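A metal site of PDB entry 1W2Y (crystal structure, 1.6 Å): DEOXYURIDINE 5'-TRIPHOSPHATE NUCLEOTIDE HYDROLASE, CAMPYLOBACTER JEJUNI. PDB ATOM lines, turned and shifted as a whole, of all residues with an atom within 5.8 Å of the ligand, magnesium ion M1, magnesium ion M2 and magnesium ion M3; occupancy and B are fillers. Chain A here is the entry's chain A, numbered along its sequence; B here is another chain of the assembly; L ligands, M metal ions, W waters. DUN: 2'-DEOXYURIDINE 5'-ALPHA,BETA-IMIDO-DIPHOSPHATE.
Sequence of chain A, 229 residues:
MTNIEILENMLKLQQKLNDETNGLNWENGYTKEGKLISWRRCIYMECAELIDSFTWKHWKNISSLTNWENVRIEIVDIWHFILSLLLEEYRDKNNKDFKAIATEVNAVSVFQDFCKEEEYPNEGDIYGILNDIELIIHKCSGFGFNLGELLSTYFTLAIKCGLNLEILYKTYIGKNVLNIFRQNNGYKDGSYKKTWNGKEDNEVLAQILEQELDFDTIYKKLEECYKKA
Leu 17 touches the ligand (CD2 to O2, 3.2 Å).
Trp 39 touches the ligand.
CB of His 80 touches C2' of the ligand, 3.4 Å away.
Phe 81 touches the ligand.
Lys 60 of chain B touches the ligand.
Hydrophobic or aromatic side chains that line the ligand: Leu 17, Trp 39, His 80, Phe 81, Tyr 187, His 58 of chain B and Trp 59 of chain B.
The nearest printed residue that does not touch the ligand is Thr 21 (4.1 Å).
Water W7 bridges an oxygen (O2B) of the ligand (2.8 Å) and the side-chain amide nitrogen (ND2) of Asn 202 (3.3 Å).
Water W1 lies within hydrogen-bond range of the side-chain amino group (NZ) of Lys 57 of chain B and a nitrogen (N3A) of the ligand.
Water W2 lies within hydrogen-bond range of O2B of the ligand and NZ of Lys 194.
Water W9 lies within hydrogen-bond range of the side-chain amide oxygen (OD1) of Asn 179 (2.8 Å), an oxygen (O4') of the ligand (2.9 Å) and the guanidinium group (NH1) of Arg 182 (2.9 Å).
NH1 of Arg 182 is in salt-bridge range of O1B of the ligand (2.9 Å).
O1B of the ligand lies within salt-bridge range of NZ of Lys 175.
The indole nitrogen of Trp 59 of chain B lies within hydrogen-bond range of an oxygen (O2A) of the ligand (2.9 Å).
O2A of the ligand lies within salt-bridge range of NZ of Lys 57 of chain B (3.0 Å).
A ring nitrogen (NE2) of His 58 of chain B lies within hydrogen-bond range of an oxygen (O4) of the ligand, at 2.9 Å.
A nitrogen (N3) of the ligand lies within hydrogen-bond range of the side-chain amide oxygen (OD1) of Asn 18, 2.9 Å away.
NE2 of Gln 14 lies within hydrogen-bond range of O2 of the ligand.
The side-chain amide nitrogen (ND2) of Asn 22 is in hydrogen-bond range of an oxygen (O4) of the ligand (2.9 Å).
The side-chain hydroxyl (OH) of Tyr 187 is in hydrogen-bond range of an oxygen (O2A) of the ligand, 2.6 Å away.
ND2 of Asn 202 sits at hydrogen-bond distance from O2B of the ligand.
NZ of Lys 194 is in salt-bridge range of O2B of the ligand (2.7 Å).
The side-chain amide nitrogen (ND2) of Asn 179 lies within hydrogen-bond range of an oxygen (O3') of the ligand (2.9 Å).
Magnesium ion M1 is bound by the side-chain carboxylate (OE1) of Glu 46, the side-chain carboxylate (OE1) of Glu 74, an oxygen (O3B) of the ligand, the side-chain carboxylate (OE2) of Glu 49, the side-chain carboxylate (OD2) of Asp 77 and water W7.
Magnesium ion M1 has six donor atoms within binding distance.
Magnesium ion M3 is bound by water W3 (1.9 Å), water W2 (2.0 Å), OE2 of Glu 74 (2.1 Å), OE2 of Glu 49 (2.1 Å), water W7 (2.2 Å) and water W4 (2.2 Å).
Four residues have an atom within 4 Å of magnesium ion M1: Glu 46, Glu 49, Glu 74 and Asp 77.
The nearest printed residue that does not touch magnesium ion M1 is Lys 175 (4.8 Å).
Magnesium ion M2 is bound by an oxygen (O1A) of the ligand, the side-chain carboxylate of Glu 46, the side-chain carboxylate of Glu 49, an oxygen (O3B) of the ligand, water W1 and water W5.
ND2 of Asn 18 is in hydrogen-bond range of OG of Ser 84 (2.8 Å).
O of Lys 194 is in hydrogen-bond range of N of Asp 201, 2.8 Å away.
ND2 of Asn 179 is in hydrogen-bond range of NE2 of His 80 (3.0 Å).
The side-chain hydroxyl (OG) of Ser 84 sits at hydrogen-bond distance from the side-chain amide nitrogen (NE2) of Gln 14, at 3.2 Å.
The side-chain amide oxygen of Gln 14 sits close to the backbone carbonyl oxygen of His 80, at 3.4 Å.
ND1 of His 80 lies within hydrogen-bond range of O of Val 76 (3.0 Å).
The side-chain amino group (NZ) of Lys 175 lies within hydrogen-bond range of the side-chain amide oxygen (OD1) of Asn 202 (2.8 Å).
NE of Arg 182 is in salt-bridge range of OD2 of Asp 201, 2.8 Å away.
Residues that only touch magnesium ion M2: Lys 57 of chain B (3.9 Å).
Within 4 Å of magnesium ion M2: Glu 46, Glu 49 and Lys 57 of chain B.
The nearest printed residue that does not touch magnesium ion M2 is Asp 77 (4.8 Å).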
ATOM      1  N   GLN A  14       7.366   9.049  25.681  1.00  0.00           N
ATOM      2  CA  GLN A  14       6.071   9.260  24.978  1.00  0.00           C
ATOM      3  C   GLN A  14       5.212  10.243  25.771  1.00  0.00           C
ATOM      4  O   GLN A  14       4.577  11.142  25.191  1.00  0.00           O
ATOM      5  CB  GLN A  14       5.322   7.970  24.761  1.00  0.00           C
ATOM      6  CG  GLN A  14       4.141   8.186  23.808  1.00  0.00           C
ATOM      7  CD  GLN A  14       4.586   8.577  22.390  1.00  0.00           C
ATOM      8  OE1 GLN A  14       5.500   7.920  21.826  1.00  0.00           O
ATOM      9  NE2 GLN A  14       3.927   9.631  21.796  1.00  0.00           N
ATOM     10  N   LEU A  17       6.672  13.754  25.322  1.00  0.00           N
ATOM     11  CA  LEU A  17       6.388  14.262  23.979  1.00  0.00           C
ATOM     12  C   LEU A  17       4.898  14.638  23.825  1.00  0.00           C
ATOM     13  O   LEU A  17       4.578  15.674  23.264  1.00  0.00           O
ATOM     14  CB  LEU A  17       6.720  13.182  22.950  1.00  0.00           C
ATOM     15  CG  LEU A  17       6.314  13.481  21.519  1.00  0.00           C
ATOM     16  CD1 LEU A  17       6.957  14.699  20.917  1.00  0.00           C
ATOM     17  CD2 LEU A  17       6.587  12.249  20.697  1.00  0.00           C
ATOM     18  N   ASN A  18       3.994  13.793  24.342  1.00  0.00           N
ATOM     19  CA  ASN A  18       2.562  14.083  24.251  1.00  0.00           C
ATOM     20  C   ASN A  18       2.212  15.326  25.082  1.00  0.00           C
ATOM     21  O   ASN A  18       1.378  16.152  24.671  1.00  0.00           O
ATOM     22  CB  ASN A  18       1.705  12.898  24.664  1.00  0.00           C
ATOM     23  CG  ASN A  18       1.704  11.778  23.609  1.00  0.00           C
ATOM     24  OD1 ASN A  18       2.265  11.949  22.533  1.00  0.00           O
ATOM     25  ND2 ASN A  18       1.017  10.662  23.903  1.00  0.00           N
ATOM     26  N   THR A  21       3.516  18.297  23.065  1.00  0.00           N
ATOM     27  CA  THR A  21       2.761  18.458  21.798  1.00  0.00           C
ATOM     28  C   THR A  21       1.330  18.922  22.051  1.00  0.00           C
ATOM     29  O   THR A  21       0.802  19.815  21.361  1.00  0.00           O
ATOM     30  CB  THR A  21       2.741  17.111  21.025  1.00  0.00           C
ATOM     31  OG1 THR A  21       4.091  16.680  20.674  1.00  0.00           O
ATOM     32  CG2 THR A  21       1.946  17.206  19.678  1.00  0.00           C
ATOM     33  N   ASN A  22       0.663  18.277  23.001  1.00  0.00           N
ATOM     34  CA  ASN A  22      -0.787  18.400  23.187  1.00  0.00           C
ATOM     35  C   ASN A  22      -1.271  19.168  24.409  1.00  0.00           C
ATOM     36  O   ASN A  22      -2.476  19.445  24.564  1.00  0.00           O
ATOM     37  CB  ASN A  22      -1.331  17.004  23.305  1.00  0.00           C
ATOM     38  CG  ASN A  22      -1.010  16.173  22.090  1.00  0.00           C
ATOM     39  OD1 ASN A  22      -1.230  16.600  20.958  1.00  0.00           O
ATOM     40  ND2 ASN A  22      -0.446  14.973  22.333  1.00  0.00           N
ATOM     41  N   TRP A  39      -6.175   7.978  19.053  1.00  0.00           N
ATOM     42  CA  TRP A  39      -4.948   7.211  18.869  1.00  0.00           C
ATOM     43  C   TRP A  39      -5.163   6.026  17.911  1.00  0.00           C
ATOM     44  O   TRP A  39      -4.248   5.659  17.162  1.00  0.00           O
ATOM     45  CB  TRP A  39      -4.442   6.690  20.178  1.00  0.00           C
ATOM     46  CG  TRP A  39      -4.097   7.788  21.131  1.00  0.00           C
ATOM     47  CD1 TRP A  39      -4.640   7.978  22.339  1.00  0.00           C
ATOM     48  CD2 TRP A  39      -3.158   8.855  20.940  1.00  0.00           C
ATOM     49  NE1 TRP A  39      -4.109   9.083  22.963  1.00  0.00           N
ATOM     50  CE2 TRP A  39      -3.189   9.655  22.120  1.00  0.00           C
ATOM     51  CE3 TRP A  39      -2.283   9.214  19.918  1.00  0.00           C
ATOM     52  CZ2 TRP A  39      -2.351  10.756  22.304  1.00  0.00           C
ATOM     53  CZ3 TRP A  39      -1.473  10.380  20.055  1.00  0.00           C
ATOM     54  CH2 TRP A  39      -1.511  11.120  21.271  1.00  0.00           C
ATOM     55  N   CYS A  42      -4.843   7.336  14.519  1.00  0.00           N
ATOM     56  CA  CYS A  42      -3.404   7.563  14.275  1.00  0.00           C
ATOM     57  C   CYS A  42      -2.720   6.257  13.826  1.00  0.00           C
ATOM     58  O   CYS A  42      -1.890   6.244  12.915  1.00  0.00           O
ATOM     59  CB  CYS A  42      -2.764   8.125  15.553  1.00  0.00           C
ATOM     60  SG  CYS A  42      -3.261   9.813  15.911  1.00  0.00           S
ATOM     61  N   MET A  45      -3.774   4.943  10.327  1.00  0.00           N
ATOM     62  CA  MET A  45      -3.206   5.826   9.266  1.00  0.00           C
ATOM     63  C   MET A  45      -1.723   5.497   9.081  1.00  0.00           C
ATOM     64  O   MET A  45      -1.203   5.489   7.949  1.00  0.00           O
ATOM     65  CB  MET A  45      -3.481   7.275   9.585  1.00  0.00           C
ATOM     66  CG  MET A  45      -4.952   7.640   9.480  1.00  0.00           C
ATOM     67  SD  MET A  45      -5.636   7.432   7.825  1.00  0.00           S
ATOM     68  CE  MET A  45      -4.897   8.883   7.070  1.00  0.00           C
ATOM     69  N   GLU A  46      -0.983   5.212  10.171  1.00  0.00           N
ATOM     70  CA  GLU A  46       0.428   4.778   9.998  1.00  0.00           C
ATOM     71  C   GLU A  46       0.468   3.398   9.374  1.00  0.00           C
ATOM     72  O   GLU A  46       1.409   3.076   8.659  1.00  0.00           O
ATOM     73  CB  GLU A  46       1.180   4.792  11.319  1.00  0.00           C
ATOM     74  CG  GLU A  46       1.313   6.191  11.955  1.00  0.00           C
ATOM     75  CD  GLU A  46       2.070   7.167  11.092  1.00  0.00           C
ATOM     76  OE1 GLU A  46       3.082   6.720  10.432  1.00  0.00           O
ATOM     77  OE2 GLU A  46       1.715   8.363  11.107  1.00  0.00           O
ATOM     78  N   GLU A  49       0.557   3.937   5.788  1.00  0.00           N
ATOM     79  CA  GLU A  49       1.918   4.292   5.398  1.00  0.00           C
ATOM     80  C   GLU A  49       2.819   3.090   5.336  1.00  0.00           C
ATOM     81  O   GLU A  49       3.639   2.986   4.432  1.00  0.00           O
ATOM     82  CB  GLU A  49       2.532   5.271   6.386  1.00  0.00           C
ATOM     83  CG  GLU A  49       1.874   6.656   6.340  1.00  0.00           C
ATOM     84  CD  GLU A  49       2.488   7.547   7.400  1.00  0.00           C
ATOM     85  OE1 GLU A  49       1.705   8.188   8.121  1.00  0.00           O
ATOM     86  OE2 GLU A  49       3.740   7.539   7.552  1.00  0.00           O
ATOM     87  N   ASN A  70      11.827   2.406   5.229  1.00  0.00           N
ATOM     88  CA  ASN A  70      10.579   3.056   5.619  1.00  0.00           C
ATOM     89  C   ASN A  70       9.729   2.117   6.436  1.00  0.00           C
ATOM     90  O   ASN A  70       9.031   2.544   7.334  1.00  0.00           O
ATOM     91  CB  ASN A  70       9.778   3.587   4.433  1.00  0.00           C
ATOM     92  CG  ASN A  70       8.817   4.679   4.887  1.00  0.00           C
ATOM     93  OD1 ASN A  70       9.288   5.731   5.371  1.00  0.00           O
ATOM     94  ND2 ASN A  70       7.510   4.417   4.839  1.00  0.00           N
ATOM     95  N   ILE A  73      10.659   2.798   9.997  1.00  0.00           N
ATOM     96  CA  ILE A  73      10.080   4.088  10.427  1.00  0.00           C
ATOM     97  C   ILE A  73       8.576   3.967  10.766  1.00  0.00           C
ATOM     98  O   ILE A  73       8.118   4.463  11.787  1.00  0.00           O
ATOM     99  CB  ILE A  73      10.256   5.099   9.286  1.00  0.00           C
ATOM    100  CG1 ILE A  73      11.743   5.501   9.130  1.00  0.00           C
ATOM    101  CG2 ILE A  73       9.343   6.228   9.380  1.00  0.00           C
ATOM    102  CD1 ILE A  73      12.465   6.040  10.416  1.00  0.00           C
ATOM    103  N   GLU A  74       7.813   3.272   9.913  1.00  0.00           N
ATOM    104  CA  GLU A  74       6.375   3.216  10.138  1.00  0.00           C
ATOM    105  C   GLU A  74       6.055   2.319  11.342  1.00  0.00           C
ATOM    106  O   GLU A  74       5.108   2.592  12.107  1.00  0.00           O
ATOM    107  CB  GLU A  74       5.612   2.821   8.896  1.00  0.00           C
ATOM    108  CG  GLU A  74       5.937   3.630   7.681  1.00  0.00           C
ATOM    109  CD  GLU A  74       5.734   5.139   7.812  1.00  0.00           C
ATOM    110  OE1 GLU A  74       5.243   5.622   8.859  1.00  0.00           O
ATOM    111  OE2 GLU A  74       6.042   5.841   6.817  1.00  0.00           O
ATOM    112  N   VAL A  76       7.878   2.128  13.913  1.00  0.00           N
ATOM    113  CA  VAL A  76       8.164   3.023  15.040  1.00  0.00           C
ATOM    114  C   VAL A  76       7.082   4.086  15.243  1.00  0.00           C
ATOM    115  O   VAL A  76       6.723   4.396  16.408  1.00  0.00           O
ATOM    116  CB  VAL A  76       9.554   3.640  14.830  1.00  0.00           C
ATOM    117  CG1 VAL A  76       9.769   4.776  15.746  1.00  0.00           C
ATOM    118  CG2 VAL A  76      10.624   2.504  15.031  1.00  0.00           C
ATOM    119  N   ASP A  77       6.522   4.610  14.149  1.00  0.00           N
ATOM    120  CA  ASP A  77       5.406   5.553  14.269  1.00  0.00           C
ATOM    121  C   ASP A  77       4.179   4.884  14.938  1.00  0.00           C
ATOM    122  O   ASP A  77       3.542   5.430  15.839  1.00  0.00           O
ATOM    123  CB  ASP A  77       5.005   6.113  12.904  1.00  0.00           C
ATOM    124  CG  ASP A  77       5.989   7.099  12.343  1.00  0.00           C
ATOM    125  OD1 ASP A  77       6.858   7.568  13.113  1.00  0.00           O
ATOM    126  OD2 ASP A  77       5.960   7.455  11.141  1.00  0.00           O
ATOM    127  N   HIS A  80       4.758   4.728  18.706  1.00  0.00           N
ATOM    128  CA  HIS A  80       4.491   5.991  19.402  1.00  0.00           C
ATOM    129  C   HIS A  80       2.998   6.047  19.776  1.00  0.00           C
ATOM    130  O   HIS A  80       2.610   6.442  20.909  1.00  0.00           O
ATOM    131  CB  HIS A  80       4.799   7.230  18.552  1.00  0.00           C
ATOM    132  CG  HIS A  80       6.242   7.654  18.503  1.00  0.00           C
ATOM    133  ND1 HIS A  80       7.206   6.947  17.816  1.00  0.00           N
ATOM    134  CD2 HIS A  80       6.861   8.766  19.009  1.00  0.00           C
ATOM    135  CE1 HIS A  80       8.352   7.622  17.867  1.00  0.00           C
ATOM    136  NE2 HIS A  80       8.186   8.708  18.616  1.00  0.00           N
ATOM    137  N   PHE A  81       2.146   5.630  18.824  1.00  0.00           N
ATOM    138  CA  PHE A  81       0.722   5.710  19.062  1.00  0.00           C
ATOM    139  C   PHE A  81       0.190   4.611  19.957  1.00  0.00           C
ATOM    140  O   PHE A  81      -0.751   4.820  20.758  1.00  0.00           O
ATOM    141  CB  PHE A  81      -0.002   5.797  17.727  1.00  0.00           C
ATOM    142  CG  PHE A  81       0.305   7.056  16.944  1.00  0.00           C
ATOM    143  CD1 PHE A  81       0.135   8.305  17.538  1.00  0.00           C
ATOM    144  CD2 PHE A  81       0.762   7.019  15.615  1.00  0.00           C
ATOM    145  CE1 PHE A  81       0.310   9.476  16.850  1.00  0.00           C
ATOM    146  CE2 PHE A  81       0.960   8.191  14.928  1.00  0.00           C
ATOM    147  CZ  PHE A  81       0.754   9.411  15.555  1.00  0.00           C
ATOM    148  N   SER A  84       1.034   5.748  23.371  1.00  0.00           N
ATOM    149  CA  SER A  84       0.031   6.770  23.702  1.00  0.00           C
ATOM    150  C   SER A  84      -1.264   6.137  24.191  1.00  0.00           C
ATOM    151  O   SER A  84      -1.807   6.530  25.233  1.00  0.00           O
ATOM    152  CB  SER A  84      -0.168   7.694  22.531  1.00  0.00           C
ATOM    153  OG  SER A  84       1.024   8.404  22.170  1.00  0.00           O
ATOM    154  N   LYS A 175      13.213   8.941  16.313  1.00  0.00           N
ATOM    155  CA  LYS A 175      11.958   9.508  15.825  1.00  0.00           C
ATOM    156  C   LYS A 175      11.287  10.409  16.906  1.00  0.00           C
ATOM    157  O   LYS A 175      10.717  11.427  16.555  1.00  0.00           O
ATOM    158  CB  LYS A 175      11.014   8.413  15.328  1.00  0.00           C
ATOM    159  CG  LYS A 175       9.696   8.948  14.653  1.00  0.00           C
ATOM    160  CD  LYS A 175       9.907  10.082  13.638  1.00  0.00           C
ATOM    161  CE  LYS A 175       8.658  10.525  12.872  1.00  0.00           C
ATOM    162  NZ  LYS A 175       8.234   9.546  11.861  1.00  0.00           N
ATOM    163  N   ASN A 179      10.160  14.144  16.230  1.00  0.00           N
ATOM    164  CA  ASN A 179       8.819  14.579  16.582  1.00  0.00           C
ATOM    165  C   ASN A 179       8.803  15.900  17.378  1.00  0.00           C
ATOM    166  O   ASN A 179       7.974  16.788  17.126  1.00  0.00           O
ATOM    167  CB  ASN A 179       8.063  13.477  17.321  1.00  0.00           C
ATOM    168  CG  ASN A 179       7.576  12.395  16.395  1.00  0.00           C
ATOM    169  OD1 ASN A 179       7.225  12.688  15.244  1.00  0.00           O
ATOM    170  ND2 ASN A 179       7.540  11.127  16.880  1.00  0.00           N
ATOM    171  N   ARG A 182      10.014  18.715  14.904  1.00  0.00           N
ATOM    172  CA  ARG A 182       8.889  19.163  14.073  1.00  0.00           C
ATOM    173  C   ARG A 182       8.022  20.175  14.821  1.00  0.00           C
ATOM    174  O   ARG A 182       7.657  21.202  14.286  1.00  0.00           O
ATOM    175  CB  ARG A 182       8.019  17.949  13.724  1.00  0.00           C
ATOM    176  CG  ARG A 182       8.582  17.082  12.626  1.00  0.00           C
ATOM    177  CD  ARG A 182       7.766  15.813  12.453  1.00  0.00           C
ATOM    178  NE  ARG A 182       8.145  14.972  11.331  1.00  0.00           N
ATOM    179  CZ  ARG A 182       7.628  13.786  11.111  1.00  0.00           C
ATOM    180  NH1 ARG A 182       6.644  13.307  11.902  1.00  0.00           N
ATOM    181  NH2 ARG A 182       8.040  13.060  10.092  1.00  0.00           N
ATOM    182  N   TYR A 187       5.355  22.629  12.817  1.00  0.00           N
ATOM    183  CA  TYR A 187       4.512  21.525  12.364  1.00  0.00           C
ATOM    184  C   TYR A 187       2.998  21.850  12.484  1.00  0.00           C
ATOM    185  O   TYR A 187       2.207  21.494  11.581  1.00  0.00           O
ATOM    186  CB  TYR A 187       4.825  20.207  13.112  1.00  0.00           C
ATOM    187  CG  TYR A 187       4.675  18.952  12.263  1.00  0.00           C
ATOM    188  CD1 TYR A 187       5.442  18.775  11.121  1.00  0.00           C
ATOM    189  CD2 TYR A 187       3.810  17.960  12.641  1.00  0.00           C
ATOM    190  CE1 TYR A 187       5.351  17.624  10.393  1.00  0.00           C
ATOM    191  CE2 TYR A 187       3.702  16.801  11.901  1.00  0.00           C
ATOM    192  CZ  TYR A 187       4.464  16.632  10.761  1.00  0.00           C
ATOM    193  OH  TYR A 187       4.335  15.483   9.980  1.00  0.00           O
ATOM    194  N   LYS A 194       8.781  19.538   5.398  1.00  0.00           N
ATOM    195  CA  LYS A 194       8.969  18.110   5.657  1.00  0.00           C
ATOM    196  C   LYS A 194       9.996  17.464   4.710  1.00  0.00           C
ATOM    197  O   LYS A 194      10.553  16.400   5.017  1.00  0.00           O
ATOM    198  CB  LYS A 194       7.647  17.349   5.628  1.00  0.00           C
ATOM    199  CG  LYS A 194       7.701  16.044   6.417  1.00  0.00           C
ATOM    200  CD  LYS A 194       6.393  15.384   6.507  1.00  0.00           C
ATOM    201  CE  LYS A 194       6.453  14.071   7.295  1.00  0.00           C
ATOM    202  NZ  LYS A 194       5.721  13.013   6.611  1.00  0.00           N
ATOM    203  N   ASP A 201      12.171  14.253   5.962  1.00  0.00           N
ATOM    204  CA  ASP A 201      12.819  14.293   7.263  1.00  0.00           C
ATOM    205  C   ASP A 201      13.124  12.897   7.857  1.00  0.00           C
ATOM    206  O   ASP A 201      14.209  12.676   8.412  1.00  0.00           O
ATOM    207  CB  ASP A 201      12.108  15.245   8.221  1.00  0.00           C
ATOM    208  CG  ASP A 201      10.646  14.871   8.529  1.00  0.00           C
ATOM    209  OD1 ASP A 201      10.097  13.800   8.078  1.00  0.00           O
ATOM    210  OD2 ASP A 201       9.998  15.605   9.301  1.00  0.00           O
ATOM    211  N   ASN A 202      12.203  11.949   7.666  1.00  0.00           N
ATOM    212  CA  ASN A 202      12.429  10.593   8.131  1.00  0.00           C
ATOM    213  C   ASN A 202      13.671   9.965   7.519  1.00  0.00           C
ATOM    214  O   ASN A 202      14.352   9.180   8.191  1.00  0.00           O
ATOM    215  CB  ASN A 202      11.229   9.707   7.818  1.00  0.00           C
ATOM    216  CG  ASN A 202      10.035  10.029   8.707  1.00  0.00           C
ATOM    217  OD1 ASN A 202      10.198  10.069   9.933  1.00  0.00           O
ATOM    218  ND2 ASN A 202       8.846  10.303   8.118  1.00  0.00           N
ATOM    219  N   LYS B  57      -5.546  15.437  11.822  1.00  0.00           N
ATOM    220  CA  LYS B  57      -4.411  15.327  12.708  1.00  0.00           C
ATOM    221  C   LYS B  57      -4.489  16.398  13.768  1.00  0.00           C
ATOM    222  O   LYS B  57      -4.729  17.579  13.464  1.00  0.00           O
ATOM    223  CB  LYS B  57      -3.094  15.459  11.918  1.00  0.00           C
ATOM    224  CG  LYS B  57      -2.744  14.248  11.053  1.00  0.00           C
ATOM    225  CD  LYS B  57      -1.357  14.326  10.481  1.00  0.00           C
ATOM    226  CE  LYS B  57      -0.968  13.114   9.721  1.00  0.00           C
ATOM    227  NZ  LYS B  57       0.376  13.146   9.084  1.00  0.00           N
ATOM    228  N   HIS B  58      -4.297  16.018  15.034  1.00  0.00           N
ATOM    229  CA  HIS B  58      -4.392  16.965  16.124  1.00  0.00           C
ATOM    230  C   HIS B  58      -3.085  17.738  16.383  1.00  0.00           C
ATOM    231  O   HIS B  58      -3.001  18.572  17.288  1.00  0.00           O
ATOM    232  CB  HIS B  58      -4.838  16.280  17.427  1.00  0.00           C
ATOM    233  CG  HIS B  58      -3.929  15.184  17.867  1.00  0.00           C
ATOM    234  ND1 HIS B  58      -4.129  13.848  17.522  1.00  0.00           N
ATOM    235  CD2 HIS B  58      -2.793  15.221  18.625  1.00  0.00           C
ATOM    236  CE1 HIS B  58      -3.147  13.130  18.061  1.00  0.00           C
ATOM    237  NE2 HIS B  58      -2.334  13.940  18.738  1.00  0.00           N
ATOM    238  N   TRP B  59      -2.035  17.332  15.642  1.00  0.00           N
ATOM    239  CA  TRP B  59      -0.697  17.836  15.855  1.00  0.00           C
ATOM    240  C   TRP B  59      -0.034  18.509  14.664  1.00  0.00           C
ATOM    241  O   TRP B  59       1.153  18.866  14.760  1.00  0.00           O
ATOM    242  CB  TRP B  59       0.236  16.691  16.316  1.00  0.00           C
ATOM    243  CG  TRP B  59       0.539  15.669  15.269  1.00  0.00           C
ATOM    244  CD1 TRP B  59       1.682  15.589  14.490  1.00  0.00           C
ATOM    245  CD2 TRP B  59      -0.264  14.543  14.915  1.00  0.00           C
ATOM    246  NE1 TRP B  59       1.603  14.493  13.653  1.00  0.00           N
ATOM    247  CE2 TRP B  59       0.411  13.844  13.896  1.00  0.00           C
ATOM    248  CE3 TRP B  59      -1.531  14.072  15.333  1.00  0.00           C
ATOM    249  CZ2 TRP B  59      -0.085  12.648  13.354  1.00  0.00           C
ATOM    250  CZ3 TRP B  59      -2.023  12.918  14.771  1.00  0.00           C
ATOM    251  CH2 TRP B  59      -1.318  12.222  13.764  1.00  0.00           C
ATOM    252  N   LYS B  60      -0.761  18.651  13.559  1.00  0.00           N
ATOM    253  CA  LYS B  60      -0.140  19.087  12.305  1.00  0.00           C
ATOM    254  C   LYS B  60      -1.111  19.941  11.553  1.00  0.00           C
ATOM    255  O   LYS B  60      -2.261  19.542  11.324  1.00  0.00           O
ATOM    256  CB  LYS B  60       0.221  17.889  11.403  1.00  0.00           C
ATOM    257  CG  LYS B  60       1.059  18.260  10.175  1.00  0.00           C
ATOM    258  CD  LYS B  60       1.293  17.050   9.253  1.00  0.00           C
ATOM    259  CE  LYS B  60       2.228  17.423   8.113  1.00  0.00           C
ATOM    260  NZ  LYS B  60       2.466  16.316   7.114  1.00  0.00           N
HETATM  261  N1  DUN L   1       2.984  11.925  17.463  1.00  0.00           N
HETATM  262  C2  DUN L   1       3.055  11.690  18.822  1.00  0.00           C
HETATM  263  N3  DUN L   1       2.120  12.222  19.622  1.00  0.00           N
HETATM  264  C4  DUN L   1       1.085  12.984  19.173  1.00  0.00           C
HETATM  265  C5  DUN L   1       0.998  13.214  17.792  1.00  0.00           C
HETATM  266  C6  DUN L   1       1.972  12.692  16.997  1.00  0.00           C
HETATM  267  O2  DUN L   1       4.004  10.966  19.245  1.00  0.00           O
HETATM  268  O4  DUN L   1       0.244  13.458  19.953  1.00  0.00           O
HETATM  269  C1' DUN L   1       4.018  11.386  16.585  1.00  0.00           C
HETATM  270  C2' DUN L   1       4.135   9.872  16.561  1.00  0.00           C
HETATM  271  C3' DUN L   1       4.654   9.575  15.180  1.00  0.00           C
HETATM  272  C4' DUN L   1       4.492  10.889  14.377  1.00  0.00           C
HETATM  273  O4' DUN L   1       3.816  11.813  15.237  1.00  0.00           O
HETATM  274  O3' DUN L   1       6.057   9.230  15.277  1.00  0.00           O
HETATM  275  C5' DUN L   1       3.745  10.779  13.074  1.00  0.00           C
HETATM  276  O5' DUN L   1       3.658  12.114  12.486  1.00  0.00           O
HETATM  277  PA  DUN L   1       3.041  12.283  11.022  1.00  0.00           P
HETATM  278  O1A DUN L   1       1.975  11.232  10.798  1.00  0.00           O
HETATM  279  O2A DUN L   1       2.644  13.733  11.005  1.00  0.00           O
HETATM  280  PB  DUN L   1       5.118  10.715   9.627  1.00  0.00           P
HETATM  281  O1B DUN L   1       6.117  10.682  10.814  1.00  0.00           O
HETATM  282  O2B DUN L   1       5.810  10.872   8.327  1.00  0.00           O
HETATM  283  O3B DUN L   1       4.145   9.529   9.673  1.00  0.00           O
HETATM  284  N3A DUN L   1       4.304  12.123   9.909  1.00  0.00           N
HETATM  285 MG    MG M   1       4.668   7.519   9.452  1.00  0.00          MG
HETATM  286 MG    MG M   2       2.026   9.658   9.579  1.00  0.00          MG
HETATM  287 MG    MG M   3       5.465   7.804   6.301  1.00  0.00          MG
HETATM  288  O   HOH W   1       2.017  11.031   7.859  1.00  0.00           O
HETATM  289  O   HOH W   2       5.217   9.806   6.017  1.00  0.00           O
HETATM  290  O   HOH W   3       4.804   7.467   4.594  1.00  0.00           O
HETATM  291  O   HOH W   4       7.561   7.898   5.489  1.00  0.00           O
HETATM  292  O   HOH W   5      -0.190   9.944   9.479  1.00  0.00           O
HETATM  293  O   HOH W   6       4.390  14.702  18.417  1.00  0.00           O
HETATM  294  O   HOH W   7       6.389   8.180   8.279  1.00  0.00           O
HETATM  295  O   HOH W   8       3.019  13.689   7.132  1.00  0.00           O
HETATM  296  O   HOH W   9       5.118  14.190  14.236  1.00  0.00           O
